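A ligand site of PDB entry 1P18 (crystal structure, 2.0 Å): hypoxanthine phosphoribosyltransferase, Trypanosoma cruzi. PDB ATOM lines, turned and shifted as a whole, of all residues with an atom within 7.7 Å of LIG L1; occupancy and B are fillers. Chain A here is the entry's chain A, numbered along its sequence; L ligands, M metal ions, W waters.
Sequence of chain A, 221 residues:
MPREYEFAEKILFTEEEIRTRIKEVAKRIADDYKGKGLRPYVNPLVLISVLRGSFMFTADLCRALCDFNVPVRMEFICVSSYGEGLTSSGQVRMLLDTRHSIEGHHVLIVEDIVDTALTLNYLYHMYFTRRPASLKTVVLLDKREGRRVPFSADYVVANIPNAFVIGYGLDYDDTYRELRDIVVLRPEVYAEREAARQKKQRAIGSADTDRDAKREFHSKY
NZ of Lys 143 is in hydrogen-bond range of O1 of LIG L1. O1 of LIG L1 lies within hydrogen-bond range of N of Val 165 (3.1 Å). A nitrogen (N2) of LIG L1 lies close to the backbone carbonyl oxygen (O) of Val 165, 2.7 Å away. The backbone NH of Asp 115 lies within hydrogen-bond range of an oxygen (O6) of LG2 L2. OD1 of Asp 112 sits close to O2 of LG2 L2 (2.9 Å). O6 of LG2 L2 sits at hydrogen-bond distance from N of Thr 116, 2.9 Å away. O8 of LG2 L2 sits close to OG1 of Thr 116 (3.5 Å). NH2 of Arg 177 is in salt-bridge range of O13 of LG2 L2, 3.6 Å away.
Water W1 lies within hydrogen-bond range of O of Asp 171 and N1 of LIG L1.
N4 of LIG L1 sits close to O5 of LG2 L2 (3.0 Å).
The side-chain amino group of Lys 143 sits at hydrogen-bond distance from the backbone carbonyl oxygen of Ala 163 (3.0 Å). The side-chain amino group of Lys 143 lies within salt-bridge range of the side-chain carboxylate of Asp 115, 3.9 Å away. N of Lys 143 sits at hydrogen-bond distance from O of Val 114 (2.9 Å). The backbone NH (N) of Leu 185 sits at hydrogen-bond distance from the backbone carbonyl oxygen (O) of Phe 164, 2.7 Å away. The guanidinium group of Arg 177 lies within salt-bridge range of the side-chain carboxylate of Asp 171 (3.9 Å).
Ile 113 touches LIG L1. Asp 115 touches LIG L1 (OD2 to N3, 3.9 Å). Ala 163 touches LIG L1. Phe 164 touches LIG L1. Leu 170 touches LIG L1. Asp 171 touches LIG L1 (O to C3, 3.4 Å). Hydrophobic or aromatic side chains within 4 Å of LIG L1: Ile 113, Phe 164, Val 165 and Leu 170. Of the 23 residues printed, 8 come within 4 Å of LIG L1.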
ATOM      1  N   GLU A 111       5.666  -5.305   8.862  1.00  0.00           N
ATOM      2  CA  GLU A 111       6.161  -4.459   7.785  1.00  0.00           C
ATOM      3  C   GLU A 111       5.528  -4.945   6.519  1.00  0.00           C
ATOM      4  O   GLU A 111       5.117  -6.102   6.423  1.00  0.00           O
ATOM      5  CB  GLU A 111       7.695  -4.520   7.669  1.00  0.00           C
ATOM      6  CG  GLU A 111       8.442  -3.329   8.284  1.00  0.00           C
ATOM      7  CD  GLU A 111       8.407  -2.016   7.465  1.00  0.00           C
ATOM      8  OE1 GLU A 111       9.357  -1.222   7.607  1.00  0.00           O
ATOM      9  OE2 GLU A 111       7.450  -1.725   6.694  1.00  0.00           O
ATOM     10  N   ASP A 112       5.386  -4.049   5.564  1.00  0.00           N
ATOM     11  CA  ASP A 112       4.772  -4.392   4.289  1.00  0.00           C
ATOM     12  C   ASP A 112       5.816  -5.017   3.362  1.00  0.00           C
ATOM     13  O   ASP A 112       5.467  -5.868   2.523  1.00  0.00           O
ATOM     14  CB  ASP A 112       4.126  -3.155   3.653  1.00  0.00           C
ATOM     15  CG  ASP A 112       5.088  -1.945   3.529  1.00  0.00           C
ATOM     16  OD1 ASP A 112       6.074  -1.811   4.304  1.00  0.00           O
ATOM     17  OD2 ASP A 112       4.828  -1.080   2.675  1.00  0.00           O
ATOM     18  N   ILE A 113       7.081  -4.638   3.538  1.00  0.00           N
ATOM     19  CA  ILE A 113       8.186  -5.142   2.717  1.00  0.00           C
ATOM     20  C   ILE A 113       9.584  -5.009   3.318  1.00  0.00           C
ATOM     21  O   ILE A 113       9.952  -3.978   3.878  1.00  0.00           O
ATOM     22  CB  ILE A 113       8.191  -4.461   1.279  1.00  0.00           C
ATOM     23  CG1 ILE A 113       9.275  -5.095   0.382  1.00  0.00           C
ATOM     24  CG2 ILE A 113       8.451  -2.948   1.365  1.00  0.00           C
ATOM     25  CD1 ILE A 113       9.241  -4.630  -1.040  1.00  0.00           C
ATOM     26  N   VAL A 114      10.361  -6.085   3.214  1.00  0.00           N
ATOM     27  CA  VAL A 114      11.752  -6.053   3.661  1.00  0.00           C
ATOM     28  C   VAL A 114      12.605  -6.198   2.387  1.00  0.00           C
ATOM     29  O   VAL A 114      12.337  -7.054   1.521  1.00  0.00           O
ATOM     30  CB  VAL A 114      12.070  -7.147   4.709  1.00  0.00           C
ATOM     31  CG1 VAL A 114      11.718  -8.524   4.171  1.00  0.00           C
ATOM     32  CG2 VAL A 114      13.534  -7.071   5.133  1.00  0.00           C
ATOM     33  N   ASP A 115      13.547  -5.260   2.223  1.00  0.00           N
ATOM     34  CA  ASP A 115      14.444  -5.211   1.082  1.00  0.00           C
ATOM     35  C   ASP A 115      15.895  -5.110   1.610  1.00  0.00           C
ATOM     36  O   ASP A 115      16.516  -6.145   1.917  1.00  0.00           O
ATOM     37  CB  ASP A 115      14.074  -4.026   0.175  1.00  0.00           C
ATOM     38  CG  ASP A 115      14.920  -3.945  -1.093  1.00  0.00           C
ATOM     39  OD1 ASP A 115      15.729  -4.865  -1.365  1.00  0.00           O
ATOM     40  OD2 ASP A 115      14.781  -2.972  -1.859  1.00  0.00           O
ATOM     41  N   THR A 116      16.420  -3.891   1.785  1.00  0.00           N
ATOM     42  CA  THR A 116      17.775  -3.729   2.316  1.00  0.00           C
ATOM     43  C   THR A 116      17.849  -4.138   3.785  1.00  0.00           C
ATOM     44  O   THR A 116      18.937  -4.398   4.303  1.00  0.00           O
ATOM     45  CB  THR A 116      18.270  -2.267   2.215  1.00  0.00           C
ATOM     46  OG1 THR A 116      17.669  -1.491   3.265  1.00  0.00           O
ATOM     47  CG2 THR A 116      17.849  -1.658   0.906  1.00  0.00           C
ATOM     48  N   LEU A 141       6.001  -8.708   1.767  1.00  0.00           N
ATOM     49  CA  LEU A 141       6.877  -8.997   0.646  1.00  0.00           C
ATOM     50  C   LEU A 141       8.323  -9.001   1.112  1.00  0.00           C
ATOM     51  O   LEU A 141       8.732  -8.167   1.906  1.00  0.00           O
ATOM     52  CB  LEU A 141       6.705  -7.950  -0.461  1.00  0.00           C
ATOM     53  CG  LEU A 141       5.332  -7.733  -1.126  1.00  0.00           C
ATOM     54  CD1 LEU A 141       5.467  -6.641  -2.138  1.00  0.00           C
ATOM     55  CD2 LEU A 141       4.841  -9.007  -1.803  1.00  0.00           C
ATOM     56  N   LYS A 143      12.210  -9.076  -0.492  1.00  0.00           N
ATOM     57  CA  LYS A 143      13.115  -8.964  -1.638  1.00  0.00           C
ATOM     58  C   LYS A 143      14.392  -9.565  -1.080  1.00  0.00           C
ATOM     59  O   LYS A 143      15.327  -8.838  -0.724  1.00  0.00           O
ATOM     60  CB  LYS A 143      13.400  -7.511  -1.995  1.00  0.00           C
ATOM     61  CG  LYS A 143      12.796  -7.088  -3.281  1.00  0.00           C
ATOM     62  CD  LYS A 143      12.939  -5.591  -3.472  1.00  0.00           C
ATOM     63  CE  LYS A 143      11.689  -5.040  -4.144  1.00  0.00           C
ATOM     64  NZ  LYS A 143      11.728  -3.566  -4.208  1.00  0.00           N
ATOM     65  N   ILE A 160       9.800 -11.815  -3.547  1.00  0.00           N
ATOM     66  CA  ILE A 160       9.630 -11.171  -4.841  1.00  0.00           C
ATOM     67  C   ILE A 160      10.979 -10.811  -5.408  1.00  0.00           C
ATOM     68  O   ILE A 160      11.951 -10.644  -4.658  1.00  0.00           O
ATOM     69  CB  ILE A 160       8.760  -9.862  -4.747  1.00  0.00           C
ATOM     70  CG1 ILE A 160       9.383  -8.883  -3.747  1.00  0.00           C
ATOM     71  CG2 ILE A 160       7.315 -10.174  -4.321  1.00  0.00           C
ATOM     72  CD1 ILE A 160       8.863  -7.472  -3.884  1.00  0.00           C
ATOM     73  N   PRO A 161      11.068 -10.717  -6.739  1.00  0.00           N
ATOM     74  CA  PRO A 161      12.341 -10.345  -7.380  1.00  0.00           C
ATOM     75  C   PRO A 161      12.623  -8.891  -7.014  1.00  0.00           C
ATOM     76  O   PRO A 161      11.855  -8.267  -6.271  1.00  0.00           O
ATOM     77  CB  PRO A 161      12.016 -10.479  -8.871  1.00  0.00           C
ATOM     78  CG  PRO A 161      10.801 -11.396  -8.925  1.00  0.00           C
ATOM     79  CD  PRO A 161      10.005 -10.948  -7.743  1.00  0.00           C
ATOM     80  N   ASN A 162      13.654  -8.305  -7.574  1.00  0.00           N
ATOM     81  CA  ASN A 162      13.947  -6.928  -7.257  1.00  0.00           C
ATOM     82  C   ASN A 162      13.218  -5.916  -8.122  1.00  0.00           C
ATOM     83  O   ASN A 162      13.801  -4.936  -8.589  1.00  0.00           O
ATOM     84  CB  ASN A 162      15.459  -6.670  -7.202  1.00  0.00           C
ATOM     85  CG  ASN A 162      16.036  -6.994  -5.835  1.00  0.00           C
ATOM     86  OD1 ASN A 162      16.083  -8.152  -5.424  1.00  0.00           O
ATOM     87  ND2 ASN A 162      16.451  -5.954  -5.095  1.00  0.00           N
ATOM     88  N   ALA A 163      11.929  -6.124  -8.299  1.00  0.00           N
ATOM     89  CA  ALA A 163      11.102  -5.194  -9.061  1.00  0.00           C
ATOM     90  C   ALA A 163      10.578  -4.125  -8.100  1.00  0.00           C
ATOM     91  O   ALA A 163      10.646  -4.303  -6.875  1.00  0.00           O
ATOM     92  CB  ALA A 163       9.932  -5.936  -9.692  1.00  0.00           C
ATOM     93  N   PHE A 164      10.110  -2.993  -8.617  1.00  0.00           N
ATOM     94  CA  PHE A 164       9.537  -1.966  -7.751  1.00  0.00           C
ATOM     95  C   PHE A 164       8.041  -2.197  -7.793  1.00  0.00           C
ATOM     96  O   PHE A 164       7.400  -2.044  -8.844  1.00  0.00           O
ATOM     97  CB  PHE A 164       9.830  -0.530  -8.196  1.00  0.00           C
ATOM     98  CG  PHE A 164       9.449   0.477  -7.158  1.00  0.00           C
ATOM     99  CD1 PHE A 164      10.288   0.706  -6.064  1.00  0.00           C
ATOM    100  CD2 PHE A 164       8.230   1.138  -7.228  1.00  0.00           C
ATOM    101  CE1 PHE A 164       9.902   1.572  -5.033  1.00  0.00           C
ATOM    102  CE2 PHE A 164       7.843   2.004  -6.197  1.00  0.00           C
ATOM    103  CZ  PHE A 164       8.680   2.216  -5.103  1.00  0.00           C
ATOM    104  N   VAL A 165       7.521  -2.650  -6.669  1.00  0.00           N
ATOM    105  CA  VAL A 165       6.111  -2.988  -6.522  1.00  0.00           C
ATOM    106  C   VAL A 165       5.340  -1.842  -5.871  1.00  0.00           C
ATOM    107  O   VAL A 165       5.901  -1.039  -5.122  1.00  0.00           O
ATOM    108  CB  VAL A 165       5.950  -4.266  -5.679  1.00  0.00           C
ATOM    109  CG1 VAL A 165       6.465  -5.460  -6.453  1.00  0.00           C
ATOM    110  CG2 VAL A 165       6.739  -4.149  -4.384  1.00  0.00           C
ATOM    111  N   ILE A 166       4.053  -1.794  -6.164  1.00  0.00           N
ATOM    112  CA  ILE A 166       3.175  -0.753  -5.633  1.00  0.00           C
ATOM    113  C   ILE A 166       1.835  -1.432  -5.363  1.00  0.00           C
ATOM    114  O   ILE A 166       1.589  -2.537  -5.880  1.00  0.00           O
ATOM    115  CB  ILE A 166       2.990   0.419  -6.660  1.00  0.00           C
ATOM    116  CG1 ILE A 166       2.948  -0.135  -8.100  1.00  0.00           C
ATOM    117  CG2 ILE A 166       4.096   1.463  -6.498  1.00  0.00           C
ATOM    118  CD1 ILE A 166       2.667   0.864  -9.194  1.00  0.00           C
ATOM    119  N   GLY A 167       0.984  -0.769  -4.584  1.00  0.00           N
ATOM    120  CA  GLY A 167      -0.319  -1.350  -4.293  1.00  0.00           C
ATOM    121  C   GLY A 167      -0.295  -2.030  -2.945  1.00  0.00           C
ATOM    122  O   GLY A 167       0.766  -2.308  -2.389  1.00  0.00           O
ATOM    123  N   GLY A 169      -0.817  -0.928  -0.072  1.00  0.00           N
ATOM    124  CA  GLY A 169      -0.115  -0.119   0.908  1.00  0.00           C
ATOM    125  C   GLY A 169       1.204   0.439   0.448  1.00  0.00           C
ATOM    126  O   GLY A 169       1.657   1.470   0.989  1.00  0.00           O
ATOM    127  N   LEU A 170       1.833  -0.215  -0.527  1.00  0.00           N
ATOM    128  CA  LEU A 170       3.127   0.220  -1.033  1.00  0.00           C
ATOM    129  C   LEU A 170       2.978   1.314  -2.055  1.00  0.00           C
ATOM    130  O   LEU A 170       2.218   1.190  -3.018  1.00  0.00           O
ATOM    131  CB  LEU A 170       3.933  -0.957  -1.632  1.00  0.00           C
ATOM    132  CG  LEU A 170       4.596  -1.963  -0.679  1.00  0.00           C
ATOM    133  CD1 LEU A 170       3.605  -3.016  -0.221  1.00  0.00           C
ATOM    134  CD2 LEU A 170       5.742  -2.644  -1.386  1.00  0.00           C
ATOM    135  N   ASP A 171       3.793   2.336  -1.895  1.00  0.00           N
ATOM    136  CA  ASP A 171       3.772   3.471  -2.790  1.00  0.00           C
ATOM    137  C   ASP A 171       5.037   3.776  -3.563  1.00  0.00           C
ATOM    138  O   ASP A 171       6.138   3.272  -3.289  1.00  0.00           O
ATOM    139  CB  ASP A 171       3.466   4.727  -1.979  1.00  0.00           C
ATOM    140  CG  ASP A 171       4.642   5.155  -1.109  1.00  0.00           C
ATOM    141  OD1 ASP A 171       4.897   4.522  -0.056  1.00  0.00           O
ATOM    142  OD2 ASP A 171       5.322   6.124  -1.476  1.00  0.00           O
ATOM    143  N   TYR A 172       4.863   4.742  -4.460  1.00  0.00           N
ATOM    144  CA  TYR A 172       5.934   5.336  -5.232  1.00  0.00           C
ATOM    145  C   TYR A 172       5.544   6.811  -5.213  1.00  0.00           C
ATOM    146  O   TYR A 172       4.466   7.156  -5.691  1.00  0.00           O
ATOM    147  CB  TYR A 172       6.005   4.859  -6.677  1.00  0.00           C
ATOM    148  CG  TYR A 172       6.945   5.747  -7.465  1.00  0.00           C
ATOM    149  CD1 TYR A 172       8.241   5.976  -7.001  1.00  0.00           C
ATOM    150  CD2 TYR A 172       6.515   6.436  -8.590  1.00  0.00           C
ATOM    151  CE1 TYR A 172       9.076   6.877  -7.638  1.00  0.00           C
ATOM    152  CE2 TYR A 172       7.344   7.332  -9.233  1.00  0.00           C
ATOM    153  CZ  TYR A 172       8.627   7.546  -8.747  1.00  0.00           C
ATOM    154  OH  TYR A 172       9.469   8.439  -9.385  1.00  0.00           O
ATOM    155  N   ARG A 177      -0.867   3.553  -3.046  1.00  0.00           N
ATOM    156  CA  ARG A 177      -1.040   2.771  -1.825  1.00  0.00           C
ATOM    157  C   ARG A 177      -2.404   2.096  -1.780  1.00  0.00           C
ATOM    158  O   ARG A 177      -2.547   1.009  -1.210  1.00  0.00           O
ATOM    159  CB  ARG A 177      -0.942   3.631  -0.570  1.00  0.00           C
ATOM    160  CG  ARG A 177       0.370   4.291  -0.279  1.00  0.00           C
ATOM    161  CD  ARG A 177       0.445   4.566   1.212  1.00  0.00           C
ATOM    162  NE  ARG A 177       1.522   5.500   1.523  1.00  0.00           N
ATOM    163  CZ  ARG A 177       2.749   5.138   1.872  1.00  0.00           C
ATOM    164  NH1 ARG A 177       3.052   3.839   1.953  1.00  0.00           N
ATOM    165  NH2 ARG A 177       3.683   6.058   2.066  1.00  0.00           N
ATOM    166  N   VAL A 183       1.262  -4.775  -7.726  1.00  0.00           N
ATOM    167  CA  VAL A 183       1.715  -4.751  -9.091  1.00  0.00           C
ATOM    168  C   VAL A 183       3.126  -4.155  -9.218  1.00  0.00           C
ATOM    169  O   VAL A 183       3.688  -3.652  -8.249  1.00  0.00           O
ATOM    170  CB  VAL A 183       0.676  -4.015 -10.012  1.00  0.00           C
ATOM    171  CG1 VAL A 183      -0.711  -4.646  -9.869  1.00  0.00           C
ATOM    172  CG2 VAL A 183       0.631  -2.507  -9.711  1.00  0.00           C
ATOM    173  N   LEU A 185       5.676  -1.433 -10.876  1.00  0.00           N
ATOM    174  CA  LEU A 185       5.673  -0.137 -11.515  1.00  0.00           C
ATOM    175  C   LEU A 185       6.421  -0.187 -12.862  1.00  0.00           C
ATOM    176  O   LEU A 185       7.528  -0.714 -12.962  1.00  0.00           O
ATOM    177  CB  LEU A 185       6.283   0.923 -10.573  1.00  0.00           C
ATOM    178  CG  LEU A 185       6.318   2.395 -11.015  1.00  0.00           C
ATOM    179  CD1 LEU A 185       4.926   2.933 -11.360  1.00  0.00           C
ATOM    180  CD2 LEU A 185       6.969   3.230  -9.912  1.00  0.00           C
HETATM  181  C1  LIG L   1      10.281  -0.346  -0.254  1.00  0.00           C
HETATM  182  C2  LIG L   1       9.395  -0.223  -1.329  1.00  0.00           C
HETATM  183  N1  LIG L   1       8.277   0.569  -1.385  1.00  0.00           N
HETATM  184  C3  LIG L   1       7.592   0.285  -2.525  1.00  0.00           C
HETATM  185  N2  LIG L   1       8.031  -0.582  -3.514  1.00  0.00           N
HETATM  186  C4  LIG L   1       9.244  -1.274  -3.524  1.00  0.00           C
HETATM  187  O1  LIG L   1       9.620  -1.976  -4.459  1.00  0.00           O
HETATM  188  C5  LIG L   1       9.967  -0.976  -2.352  1.00  0.00           C
HETATM  189  N3  LIG L   1      11.264  -1.375  -2.044  1.00  0.00           N
HETATM  190  N4  LIG L   1      11.374  -0.984  -0.787  1.00  0.00           N
HETATM  191  C1  LG2 L   2       9.163   1.150   2.711  1.00  0.00           C
HETATM  192  C2  LG2 L   2       8.323   0.006   2.934  1.00  0.00           C
HETATM  193  C3  LG2 L   2       9.234  -0.747   3.973  1.00  0.00           C
HETATM  194  C4  LG2 L   2      10.648  -0.460   3.379  1.00  0.00           C
HETATM  195  C5  LG2 L   2      11.206  -1.700   2.625  1.00  0.00           C
HETATM  196  O1  LG2 L   2       8.860   2.082   3.726  1.00  0.00           O
HETATM  197  O2  LG2 L   2       7.085   0.674   3.247  1.00  0.00           O
HETATM  198  O3  LG2 L   2       9.429  -0.019   5.164  1.00  0.00           O
HETATM  199  O4  LG2 L   2      10.503   0.776   2.578  1.00  0.00           O
HETATM  200  O5  LG2 L   2      12.432  -1.564   1.913  1.00  0.00           O
HETATM  201  P1  LG2 L   2      13.931  -1.406   2.588  1.00  0.00           P
HETATM  202  O6  LG2 L   2      14.200  -2.690   3.303  1.00  0.00           O
HETATM  203  O7  LG2 L   2      13.883  -0.219   3.494  1.00  0.00           O
HETATM  204  O8  LG2 L   2      14.770  -1.219   1.376  1.00  0.00           O
HETATM  205  P2  LG2 L   2       8.827   3.625   3.162  1.00  0.00           P
HETATM  206  O9  LG2 L   2      10.167   4.237   3.260  1.00  0.00           O
HETATM  207  O10 LG2 L   2       8.316   3.546   1.779  1.00  0.00           O
HETATM  208  O11 LG2 L   2       7.840   4.171   4.119  1.00  0.00           O
HETATM  209  P3  LG2 L   2       6.394   3.919   3.997  1.00  0.00           P
HETATM  210  O12 LG2 L   2       6.002   4.111   2.561  1.00  0.00           O
HETATM  211  O13 LG2 L   2       5.774   4.981   4.807  1.00  0.00           O
HETATM  212  O14 LG2 L   2       6.014   2.558   4.566  1.00  0.00           O
HETATM  213 MG    MG M   1       6.953   4.095   0.400  1.00  0.00          MG
HETATM  214 MG    MG M   2       7.463   0.450   5.377  1.00  0.00          MG
HETATM  215  O   HOH W   1       7.940   4.001  -1.741  1.00  0.00           O
HETATM  216  O   HOH W   2       6.634   1.974   0.863  1.00  0.00           O
